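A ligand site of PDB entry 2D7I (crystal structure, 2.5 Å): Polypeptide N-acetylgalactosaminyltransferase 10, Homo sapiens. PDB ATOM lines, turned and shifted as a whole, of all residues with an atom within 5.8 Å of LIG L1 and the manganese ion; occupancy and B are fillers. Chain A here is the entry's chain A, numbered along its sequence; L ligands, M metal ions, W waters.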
ATOM      1  N   ILE A 118      20.318   1.749  -2.602  1.00  0.00           N
ATOM      2  CA  ILE A 118      20.423   2.357  -1.273  1.00  0.00           C
ATOM      3  C   ILE A 118      21.718   1.977  -0.557  1.00  0.00           C
ATOM      4  O   ILE A 118      21.869   0.874  -0.016  1.00  0.00           O
ATOM      5  CB  ILE A 118      19.222   1.970  -0.382  1.00  0.00           C
ATOM      6  CG1 ILE A 118      17.902   2.385  -1.047  1.00  0.00           C
ATOM      7  CG2 ILE A 118      19.358   2.642   0.980  1.00  0.00           C
ATOM      8  CD1 ILE A 118      16.672   1.739  -0.426  1.00  0.00           C
ATOM      9  N   PRO A 119      22.694   2.894  -0.560  1.00  0.00           N
ATOM     10  CA  PRO A 119      23.975   2.646   0.098  1.00  0.00           C
ATOM     11  C   PRO A 119      23.807   2.917   1.577  1.00  0.00           C
ATOM     12  O   PRO A 119      23.041   3.784   1.981  1.00  0.00           O
ATOM     13  CB  PRO A 119      24.892   3.673  -0.542  1.00  0.00           C
ATOM     14  CG  PRO A 119      23.958   4.847  -0.725  1.00  0.00           C
ATOM     15  CD  PRO A 119      22.716   4.186  -1.276  1.00  0.00           C
ATOM     16  N   PHE A 120      24.530   2.176   2.403  1.00  0.00           N
ATOM     17  CA  PHE A 120      24.412   2.398   3.821  1.00  0.00           C
ATOM     18  C   PHE A 120      25.683   1.959   4.545  1.00  0.00           C
ATOM     19  O   PHE A 120      26.443   1.120   4.068  1.00  0.00           O
ATOM     20  CB  PHE A 120      23.181   1.666   4.363  1.00  0.00           C
ATOM     21  CG  PHE A 120      23.326   0.191   4.467  1.00  0.00           C
ATOM     22  CD1 PHE A 120      23.923  -0.383   5.584  1.00  0.00           C
ATOM     23  CD2 PHE A 120      22.842  -0.636   3.460  1.00  0.00           C
ATOM     24  CE1 PHE A 120      24.036  -1.773   5.708  1.00  0.00           C
ATOM     25  CE2 PHE A 120      22.945  -2.031   3.564  1.00  0.00           C
ATOM     26  CZ  PHE A 120      23.545  -2.603   4.696  1.00  0.00           C
ATOM     27  N   HIS A 121      25.876   2.539   5.720  1.00  0.00           N
ATOM     28  CA  HIS A 121      27.039   2.246   6.534  1.00  0.00           C
ATOM     29  C   HIS A 121      26.623   2.404   7.979  1.00  0.00           C
ATOM     30  O   HIS A 121      26.284   3.505   8.418  1.00  0.00           O
ATOM     31  CB  HIS A 121      28.144   3.248   6.205  1.00  0.00           C
ATOM     32  CG  HIS A 121      29.328   3.143   7.095  1.00  0.00           C
ATOM     33  ND1 HIS A 121      30.254   2.126   6.995  1.00  0.00           N
ATOM     34  CD2 HIS A 121      29.717   3.898   8.157  1.00  0.00           C
ATOM     35  CE1 HIS A 121      31.162   2.259   7.950  1.00  0.00           C
ATOM     36  NE2 HIS A 121      30.858   3.327   8.666  1.00  0.00           N
ATOM     37  N   GLU A 123      24.037   1.942   9.470  1.00  0.00           N
ATOM     38  CA  GLU A 123      22.775   2.649   9.570  1.00  0.00           C
ATOM     39  C   GLU A 123      21.886   1.926  10.598  1.00  0.00           C
ATOM     40  O   GLU A 123      22.004   0.718  10.787  1.00  0.00           O
ATOM     41  CB  GLU A 123      22.106   2.676   8.196  1.00  0.00           C
ATOM     42  CG  GLU A 123      21.228   3.920   7.943  1.00  0.00           C
ATOM     43  CD  GLU A 123      22.022   5.212   8.061  1.00  0.00           C
ATOM     44  OE1 GLU A 123      23.006   5.405   7.302  1.00  0.00           O
ATOM     45  OE2 GLU A 123      21.658   6.034   8.933  1.00  0.00           O
ATOM     46  N   VAL A 150      23.250  -1.542  -0.521  1.00  0.00           N
ATOM     47  CA  VAL A 150      24.673  -1.735  -0.655  1.00  0.00           C
ATOM     48  C   VAL A 150      25.321  -1.371   0.671  1.00  0.00           C
ATOM     49  O   VAL A 150      25.321  -0.213   1.085  1.00  0.00           O
ATOM     50  CB  VAL A 150      25.246  -0.865  -1.800  1.00  0.00           C
ATOM     51  CG1 VAL A 150      26.706  -1.273  -2.123  1.00  0.00           C
ATOM     52  CG2 VAL A 150      24.365  -1.019  -3.036  1.00  0.00           C
ATOM     53  N   ASP A 152      28.255  -0.625   2.984  1.00  0.00           N
ATOM     54  CA  ASP A 152      29.610  -0.114   2.893  1.00  0.00           C
ATOM     55  C   ASP A 152      30.425  -0.508   4.123  1.00  0.00           C
ATOM     56  O   ASP A 152      30.661   0.288   5.025  1.00  0.00           O
ATOM     57  CB  ASP A 152      29.627   1.412   2.726  1.00  0.00           C
ATOM     58  CG  ASP A 152      31.028   1.957   2.525  1.00  0.00           C
ATOM     59  OD1 ASP A 152      31.923   1.175   2.154  1.00  0.00           O
ATOM     60  OD2 ASP A 152      31.235   3.177   2.726  1.00  0.00           O
ATOM     61  N   ARG A 181      35.945  -0.531   3.456  1.00  0.00           N
ATOM     62  CA  ARG A 181      35.263   0.762   3.472  1.00  0.00           C
ATOM     63  C   ARG A 181      35.515   1.459   2.143  1.00  0.00           C
ATOM     64  O   ARG A 181      36.657   1.758   1.812  1.00  0.00           O
ATOM     65  CB  ARG A 181      35.790   1.639   4.605  1.00  0.00           C
ATOM     66  CG  ARG A 181      35.035   2.955   4.772  1.00  0.00           C
ATOM     67  CD  ARG A 181      33.584   2.726   5.186  1.00  0.00           C
ATOM     68  NE  ARG A 181      32.892   3.982   5.471  1.00  0.00           N
ATOM     69  CZ  ARG A 181      33.150   4.779   6.513  1.00  0.00           C
ATOM     70  NH1 ARG A 181      34.093   4.458   7.389  1.00  0.00           N
ATOM     71  NH2 ARG A 181      32.478   5.901   6.662  1.00  0.00           N
ATOM     72  N   GLU A 182      34.449   1.712   1.390  1.00  0.00           N
ATOM     73  CA  GLU A 182      34.575   2.347   0.085  1.00  0.00           C
ATOM     74  C   GLU A 182      34.097   3.789   0.038  1.00  0.00           C
ATOM     75  O   GLU A 182      34.597   4.582  -0.753  1.00  0.00           O
ATOM     76  CB  GLU A 182      33.822   1.515  -0.962  1.00  0.00           C
ATOM     77  CG  GLU A 182      34.386   0.126  -1.154  1.00  0.00           C
ATOM     78  CD  GLU A 182      35.699   0.109  -1.959  1.00  0.00           C
ATOM     79  OE1 GLU A 182      36.490   1.074  -1.859  1.00  0.00           O
ATOM     80  OE2 GLU A 182      35.939  -0.895  -2.670  1.00  0.00           O
ATOM     81  N   GLY A 183      33.128   4.140   0.890  1.00  0.00           N
ATOM     82  CA  GLY A 183      32.604   5.495   0.892  1.00  0.00           C
ATOM     83  C   GLY A 183      31.311   5.547   0.101  1.00  0.00           C
ATOM     84  O   GLY A 183      31.106   4.729  -0.797  1.00  0.00           O
ATOM     85  N   LEU A 184      30.467   6.532   0.400  1.00  0.00           N
ATOM     86  CA  LEU A 184      29.185   6.633  -0.275  1.00  0.00           C
ATOM     87  C   LEU A 184      29.306   6.745  -1.798  1.00  0.00           C
ATOM     88  O   LEU A 184      28.553   6.101  -2.537  1.00  0.00           O
ATOM     89  CB  LEU A 184      28.379   7.807   0.298  1.00  0.00           C
ATOM     90  CG  LEU A 184      28.692   9.244  -0.114  1.00  0.00           C
ATOM     91  CD1 LEU A 184      27.904   9.604  -1.381  1.00  0.00           C
ATOM     92  CD2 LEU A 184      28.315  10.183   0.995  1.00  0.00           C
ATOM     93  N   THR A 187      30.459   3.443  -3.107  1.00  0.00           N
ATOM     94  CA  THR A 187      29.446   2.473  -2.708  1.00  0.00           C
ATOM     95  C   THR A 187      28.230   2.641  -3.620  1.00  0.00           C
ATOM     96  O   THR A 187      27.593   1.656  -3.962  1.00  0.00           O
ATOM     97  CB  THR A 187      29.049   2.638  -1.223  1.00  0.00           C
ATOM     98  OG1 THR A 187      30.215   2.462  -0.397  1.00  0.00           O
ATOM     99  CG2 THR A 187      27.993   1.612  -0.828  1.00  0.00           C
ATOM    100  N   ARG A 188      27.935   3.859  -4.041  1.00  0.00           N
ATOM    101  CA  ARG A 188      26.795   4.052  -4.944  1.00  0.00           C
ATOM    102  C   ARG A 188      27.172   3.515  -6.319  1.00  0.00           C
ATOM    103  O   ARG A 188      26.324   3.008  -7.047  1.00  0.00           O
ATOM    104  CB  ARG A 188      26.389   5.526  -5.046  1.00  0.00           C
ATOM    105  CG  ARG A 188      25.740   6.034  -3.780  1.00  0.00           C
ATOM    106  CD  ARG A 188      24.629   7.044  -4.032  1.00  0.00           C
ATOM    107  NE  ARG A 188      25.147   8.384  -4.258  1.00  0.00           N
ATOM    108  CZ  ARG A 188      24.823   9.436  -3.509  1.00  0.00           C
ATOM    109  NH1 ARG A 188      23.992   9.300  -2.498  1.00  0.00           N
ATOM    110  NH2 ARG A 188      25.350  10.631  -3.783  1.00  0.00           N
ATOM    111  N   LEU A 203      18.841   6.613  -3.320  1.00  0.00           N
ATOM    112  CA  LEU A 203      18.124   7.045  -2.117  1.00  0.00           C
ATOM    113  C   LEU A 203      19.006   6.819  -0.881  1.00  0.00           C
ATOM    114  O   LEU A 203      19.661   5.794  -0.776  1.00  0.00           O
ATOM    115  CB  LEU A 203      16.870   6.199  -1.972  1.00  0.00           C
ATOM    116  CG  LEU A 203      15.444   6.709  -2.148  1.00  0.00           C
ATOM    117  CD1 LEU A 203      15.234   7.488  -3.423  1.00  0.00           C
ATOM    118  CD2 LEU A 203      14.539   5.479  -2.133  1.00  0.00           C
ATOM    119  N   ASP A 204      19.032   7.770   0.054  1.00  0.00           N
ATOM    120  CA  ASP A 204      19.817   7.554   1.261  1.00  0.00           C
ATOM    121  C   ASP A 204      19.101   6.503   2.110  1.00  0.00           C
ATOM    122  O   ASP A 204      17.915   6.249   1.914  1.00  0.00           O
ATOM    123  CB  ASP A 204      19.974   8.847   2.022  1.00  0.00           C
ATOM    124  CG  ASP A 204      21.267   9.542   1.690  1.00  0.00           C
ATOM    125  OD1 ASP A 204      21.932   9.130   0.700  1.00  0.00           O
ATOM    126  OD2 ASP A 204      21.623  10.488   2.434  1.00  0.00           O
ATOM    127  N   SER A 205      19.815   5.889   3.041  1.00  0.00           N
ATOM    128  CA  SER A 205      19.231   4.827   3.843  1.00  0.00           C
ATOM    129  C   SER A 205      18.283   5.244   4.945  1.00  0.00           C
ATOM    130  O   SER A 205      17.826   4.402   5.719  1.00  0.00           O
ATOM    131  CB  SER A 205      20.312   3.954   4.448  1.00  0.00           C
ATOM    132  OG  SER A 205      21.232   4.738   5.194  1.00  0.00           O
ATOM    133  N   HIS A 206      17.983   6.527   5.028  1.00  0.00           N
ATOM    134  CA  HIS A 206      17.075   7.039   6.052  1.00  0.00           C
ATOM    135  C   HIS A 206      16.069   7.966   5.376  1.00  0.00           C
ATOM    136  O   HIS A 206      16.033   9.161   5.649  1.00  0.00           O
ATOM    137  CB  HIS A 206      17.836   7.802   7.153  1.00  0.00           C
ATOM    138  CG  HIS A 206      19.101   8.431   6.665  1.00  0.00           C
ATOM    139  ND1 HIS A 206      20.328   7.835   6.833  1.00  0.00           N
ATOM    140  CD2 HIS A 206      19.318   9.554   5.940  1.00  0.00           C
ATOM    141  CE1 HIS A 206      21.249   8.559   6.223  1.00  0.00           C
ATOM    142  NE2 HIS A 206      20.664   9.605   5.677  1.00  0.00           N
ATOM    143  N   ILE A 308      34.937   9.565   1.187  1.00  0.00           N
ATOM    144  CA  ILE A 308      33.802   9.124   2.001  1.00  0.00           C
ATOM    145  C   ILE A 308      32.509   9.908   1.799  1.00  0.00           C
ATOM    146  O   ILE A 308      31.427   9.321   1.670  1.00  0.00           O
ATOM    147  CB  ILE A 308      34.173   9.161   3.513  1.00  0.00           C
ATOM    148  CG1 ILE A 308      35.055   7.954   3.863  1.00  0.00           C
ATOM    149  CG2 ILE A 308      32.922   9.178   4.373  1.00  0.00           C
ATOM    150  CD1 ILE A 308      36.381   7.944   3.142  1.00  0.00           C
ATOM    151  N   TRP A 309      32.621  11.226   1.755  1.00  0.00           N
ATOM    152  CA  TRP A 309      31.459  12.065   1.631  1.00  0.00           C
ATOM    153  C   TRP A 309      31.840  13.401   0.988  1.00  0.00           C
ATOM    154  O   TRP A 309      32.989  13.831   1.083  1.00  0.00           O
ATOM    155  CB  TRP A 309      30.903  12.271   3.050  1.00  0.00           C
ATOM    156  CG  TRP A 309      29.704  13.127   3.188  1.00  0.00           C
ATOM    157  CD1 TRP A 309      28.415  12.703   3.392  1.00  0.00           C
ATOM    158  CD2 TRP A 309      29.667  14.556   3.186  1.00  0.00           C
ATOM    159  NE1 TRP A 309      27.579  13.792   3.531  1.00  0.00           N
ATOM    160  CE2 TRP A 309      28.317  14.944   3.409  1.00  0.00           C
ATOM    161  CE3 TRP A 309      30.644  15.553   3.027  1.00  0.00           C
ATOM    162  CZ2 TRP A 309      27.928  16.281   3.465  1.00  0.00           C
ATOM    163  CZ3 TRP A 309      30.242  16.886   3.085  1.00  0.00           C
ATOM    164  CH2 TRP A 309      28.904  17.236   3.309  1.00  0.00           C
ATOM    165  N   HIS A 337      13.590  12.828   4.193  1.00  0.00           N
ATOM    166  CA  HIS A 337      14.977  12.498   4.476  1.00  0.00           C
ATOM    167  C   HIS A 337      15.309  12.972   5.875  1.00  0.00           C
ATOM    168  O   HIS A 337      14.904  14.050   6.276  1.00  0.00           O
ATOM    169  CB  HIS A 337      15.922  13.177   3.479  1.00  0.00           C
ATOM    170  CG  HIS A 337      17.365  12.992   3.793  1.00  0.00           C
ATOM    171  ND1 HIS A 337      18.076  13.866   4.584  1.00  0.00           N
ATOM    172  CD2 HIS A 337      18.235  11.994   3.484  1.00  0.00           C
ATOM    173  CE1 HIS A 337      19.307  13.419   4.748  1.00  0.00           C
ATOM    174  NE2 HIS A 337      19.425  12.282   4.086  1.00  0.00           N
ATOM    175  N   ILE A 338      16.063  12.165   6.623  1.00  0.00           N
ATOM    176  CA  ILE A 338      16.455  12.541   7.970  1.00  0.00           C
ATOM    177  C   ILE A 338      17.813  13.233   7.930  1.00  0.00           C
ATOM    178  O   ILE A 338      18.818  12.585   7.661  1.00  0.00           O
ATOM    179  CB  ILE A 338      16.616  11.293   8.872  1.00  0.00           C
ATOM    180  CG1 ILE A 338      15.351  10.439   8.847  1.00  0.00           C
ATOM    181  CG2 ILE A 338      16.946  11.725  10.311  1.00  0.00           C
ATOM    182  CD1 ILE A 338      15.466   9.196   9.705  1.00  0.00           C
ATOM    183  N   TYR A 339      17.851  14.526   8.200  1.00  0.00           N
ATOM    184  CA  TYR A 339      19.132  15.238   8.233  1.00  0.00           C
ATOM    185  C   TYR A 339      19.775  15.013   9.611  1.00  0.00           C
ATOM    186  O   TYR A 339      19.159  15.252  10.649  1.00  0.00           O
ATOM    187  CB  TYR A 339      18.934  16.734   7.984  1.00  0.00           C
ATOM    188  CG  TYR A 339      18.424  17.034   6.602  1.00  0.00           C
ATOM    189  CD1 TYR A 339      17.077  16.871   6.287  1.00  0.00           C
ATOM    190  CD2 TYR A 339      19.299  17.438   5.600  1.00  0.00           C
ATOM    191  CE1 TYR A 339      16.623  17.098   5.003  1.00  0.00           C
ATOM    192  CE2 TYR A 339      18.852  17.667   4.322  1.00  0.00           C
ATOM    193  CZ  TYR A 339      17.510  17.495   4.020  1.00  0.00           C
ATOM    194  OH  TYR A 339      17.057  17.690   2.732  1.00  0.00           O
ATOM    195  N   ARG A 340      21.015  14.543   9.603  1.00  0.00           N
ATOM    196  CA  ARG A 340      21.692  14.230  10.840  1.00  0.00           C
ATOM    197  C   ARG A 340      21.962  15.426  11.721  1.00  0.00           C
ATOM    198  O   ARG A 340      22.243  16.513  11.219  1.00  0.00           O
ATOM    199  CB  ARG A 340      23.024  13.540  10.556  1.00  0.00           C
ATOM    200  CG  ARG A 340      22.921  12.233   9.781  1.00  0.00           C
ATOM    201  CD  ARG A 340      24.297  11.623   9.606  1.00  0.00           C
ATOM    202  NE  ARG A 340      24.333  10.606   8.553  1.00  0.00           N
ATOM    203  CZ  ARG A 340      24.009   9.338   8.731  1.00  0.00           C
ATOM    204  NH1 ARG A 340      23.620   8.909   9.930  1.00  0.00           N
ATOM    205  NH2 ARG A 340      24.090   8.483   7.716  1.00  0.00           N
ATOM    206  N   TYR A 345      29.324   7.953  12.107  1.00  0.00           N
ATOM    207  CA  TYR A 345      30.411   7.095  11.656  1.00  0.00           C
ATOM    208  C   TYR A 345      31.778   7.751  11.689  1.00  0.00           C
ATOM    209  O   TYR A 345      31.899   8.964  11.902  1.00  0.00           O
ATOM    210  CB  TYR A 345      30.143   6.558  10.253  1.00  0.00           C
ATOM    211  CG  TYR A 345      29.720   7.569   9.220  1.00  0.00           C
ATOM    212  CD1 TYR A 345      28.368   7.752   8.908  1.00  0.00           C
ATOM    213  CD2 TYR A 345      30.659   8.317   8.491  1.00  0.00           C
ATOM    214  CE1 TYR A 345      27.955   8.631   7.905  1.00  0.00           C
ATOM    215  CE2 TYR A 345      30.264   9.201   7.478  1.00  0.00           C
ATOM    216  CZ  TYR A 345      28.912   9.353   7.197  1.00  0.00           C
ATOM    217  OH  TYR A 345      28.497  10.221   6.203  1.00  0.00           O
HETATM  218  N1  LIG L   1      27.224   6.113   3.515  1.00  0.00           N
HETATM  219  C1  LIG L   1      28.010   5.091   2.984  1.00  0.00           C
HETATM  220  N2  LIG L   1      29.361   5.095   3.197  1.00  0.00           N
HETATM  221  C2  LIG L   1      29.965   6.100   3.915  1.00  0.00           C
HETATM  222  C3  LIG L   1      29.189   7.135   4.444  1.00  0.00           C
HETATM  223  C4  LIG L   1      27.823   7.177   4.144  1.00  0.00           C
HETATM  224  O1  LIG L   1      27.515   4.165   2.344  1.00  0.00           O
HETATM  225  O2  LIG L   1      31.177   6.068   4.086  1.00  0.00           O
HETATM  226  C5  LIG L   1      25.783   6.078   3.246  1.00  0.00           C
HETATM  227  C6  LIG L   1      24.882   6.491   4.391  1.00  0.00           C
HETATM  228  O3  LIG L   1      24.507   5.370   5.168  1.00  0.00           O
HETATM  229  C7  LIG L   1      23.712   7.131   3.667  1.00  0.00           C
HETATM  230  C8  LIG L   1      24.316   7.691   2.384  1.00  0.00           C
HETATM  231  O4  LIG L   1      25.538   7.000   2.209  1.00  0.00           O
HETATM  232  O5  LIG L   1      22.746   6.165   3.285  1.00  0.00           O
HETATM  233  C9  LIG L   1      24.564   9.203   2.399  1.00  0.00           C
HETATM  234  O6  LIG L   1      25.435   9.589   3.441  1.00  0.00           O
HETATM  235  P1  LIG L   1      24.915  10.496   4.665  1.00  0.00           P
HETATM  236  O7  LIG L   1      23.484  10.239   4.963  1.00  0.00           O
HETATM  237  O8  LIG L   1      25.783  10.286   5.845  1.00  0.00           O
HETATM  238  O9  LIG L   1      25.046  11.984   4.076  1.00  0.00           O
HETATM  239  P2  LIG L   1      24.057  13.188   4.465  1.00  0.00           P
HETATM  240  O10 LIG L   1      22.684  12.969   3.935  1.00  0.00           O
HETATM  241  O11 LIG L   1      23.940  13.339   5.932  1.00  0.00           O
HETATM  242  O12 LIG L   1      24.709  14.383   3.873  1.00  0.00           O
HETATM  243  C1  LG2 L   2      24.048  15.564   0.770  1.00  0.00           C
HETATM  244  C2  LG2 L   2      23.261  14.309   0.405  1.00  0.00           C
HETATM  245  C3  LG2 L   2      24.081  13.060   0.753  1.00  0.00           C
HETATM  246  C4  LG2 L   2      25.415  13.125   0.004  1.00  0.00           C
HETATM  247  C5  LG2 L   2      26.120  14.437   0.347  1.00  0.00           C
HETATM  248  C6  LG2 L   2      27.408  14.538  -0.477  1.00  0.00           C
HETATM  249  C7  LG2 L   2      20.827  14.645   0.481  1.00  0.00           C
HETATM  250  C8  LG2 L   2      19.574  14.578   1.348  1.00  0.00           C
HETATM  251  N1  LG2 L   2      21.957  14.283   1.097  1.00  0.00           N
HETATM  252  O1  LG2 L   2      23.281  16.714   0.415  1.00  0.00           O
HETATM  253  O2  LG2 L   2      23.366  11.891   0.357  1.00  0.00           O
HETATM  254  O3  LG2 L   2      25.176  13.082  -1.406  1.00  0.00           O
HETATM  255  O4  LG2 L   2      25.283  15.566   0.025  1.00  0.00           O
HETATM  256  O5  LG2 L   2      28.250  13.410  -0.213  1.00  0.00           O
HETATM  257  O6  LG2 L   2      20.762  14.980  -0.695  1.00  0.00           O
HETATM  258 MN    MN M   1      21.480  11.298   4.457  1.00  0.00          MN
HETATM  259  O   HOH W   1      21.527  11.968   6.413  1.00  0.00           O
HETATM  260  O   HOH W   2      22.309  15.201   7.203  1.00  0.00           O
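OH of Tyr 345 is in hydrogen-bond range of O8 of LIG L1, 2.7 Å away. An oxygen (O3) of LIG L1 sits at hydrogen-bond distance from the backbone NH of His 121. The indole nitrogen (NE1) of Trp 309 sits at hydrogen-bond distance from an oxygen (O12) of LIG L1. The guanidinium group of Arg 188 is in hydrogen-bond range of an oxygen (O3) of LG2 L2, at 3.4 Å. NH2 of Arg 181 lies within hydrogen-bond range of O2 of LIG L1 (2.9 Å). An oxygen (O3) of LIG L1 sits at hydrogen-bond distance from the side-chain carboxylate (OE1) of Glu 123 (2.6 Å). OG of Ser 205 lies within hydrogen-bond range of O5 of LIG L1, 2.8 Å away. The backbone NH (N) of Ser 205 lies within hydrogen-bond range of an oxygen (O5) of LIG L1, at 3.0 Å. NE of Arg 340 is in salt-bridge range of O8 of LIG L1 (3.1 Å). O5 of LIG L1 lies within hydrogen-bond range of O of Pro 119, at 2.7 Å. The side-chain carboxylate (OD1) of Asp 204 is in hydrogen-bond range of an oxygen (O2) of LG2 L2 (3.1 Å). OD2 of Asp 152 sits at hydrogen-bond distance from N2 of LIG L1, 2.7 Å away.
An oxygen (O10) of LIG L1 lies close to a nitrogen (N1) of LG2 L2, at 3.2 Å.
N of Phe 120 sits at hydrogen-bond distance from O of Val 150. The side-chain carboxylate (OD1) of Asp 152 is in hydrogen-bond range of the backbone NH (N) of Glu 182 (2.7 Å). A ring nitrogen (ND1) of His 206 sits at hydrogen-bond distance from the side-chain carboxylate of Glu 123 (3.1 Å). The backbone carbonyl oxygen (O) of Gly 183 sits at hydrogen-bond distance from the side-chain hydroxyl (OG1) of Thr 187, 2.5 Å away. OE1 of Glu 123 is in hydrogen-bond range of OG of Ser 205 (2.8 Å). OD2 of Asp 152 is in hydrogen-bond range of N of Gly 183. The side-chain carboxylate (OD1) of Asp 152 lies close to the side-chain hydroxyl (OG1) of Thr 187 (3.3 Å). The backbone carbonyl oxygen (O) of Asp 152 lies within hydrogen-bond range of a ring nitrogen (ND1) of His 121, 2.7 Å away.
N of Leu 184 sits close to N2 of LIG L1, 3.3 Å away. Phe 120 touches LIG L1 (CA to O3, 3.3 Å). Gly 183 touches LIG L1 (CA to O2, 3.5 Å). Ile 308 touches LIG L1. Of the 24 residues printed, 16 come within 4 Å of LIG L1.
Within 4 Å of the manganese ion: Asp 204, His 206 and His 337.
The manganese ion is bound by water W1 (2.1 Å), an oxygen (O10) of LIG L1 (2.1 Å), the side-chain carboxylate (OD2) of Asp 204 (2.2 Å), a ring nitrogen (NE2) of His 206 (2.2 Å), a ring nitrogen (NE2) of His 337 (2.3 Å) and an oxygen (O7) of LIG L1 (2.3 Å). The manganese ion has six donor atoms within binding distance.
Water W1 lies within hydrogen-bond range of an oxygen (O11) of LIG L1 (2.8 Å) and the backbone carbonyl oxygen (O) of Ile 338 (3.0 Å). Water W2 bridges O11 of LIG L1 and N of Arg 340.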
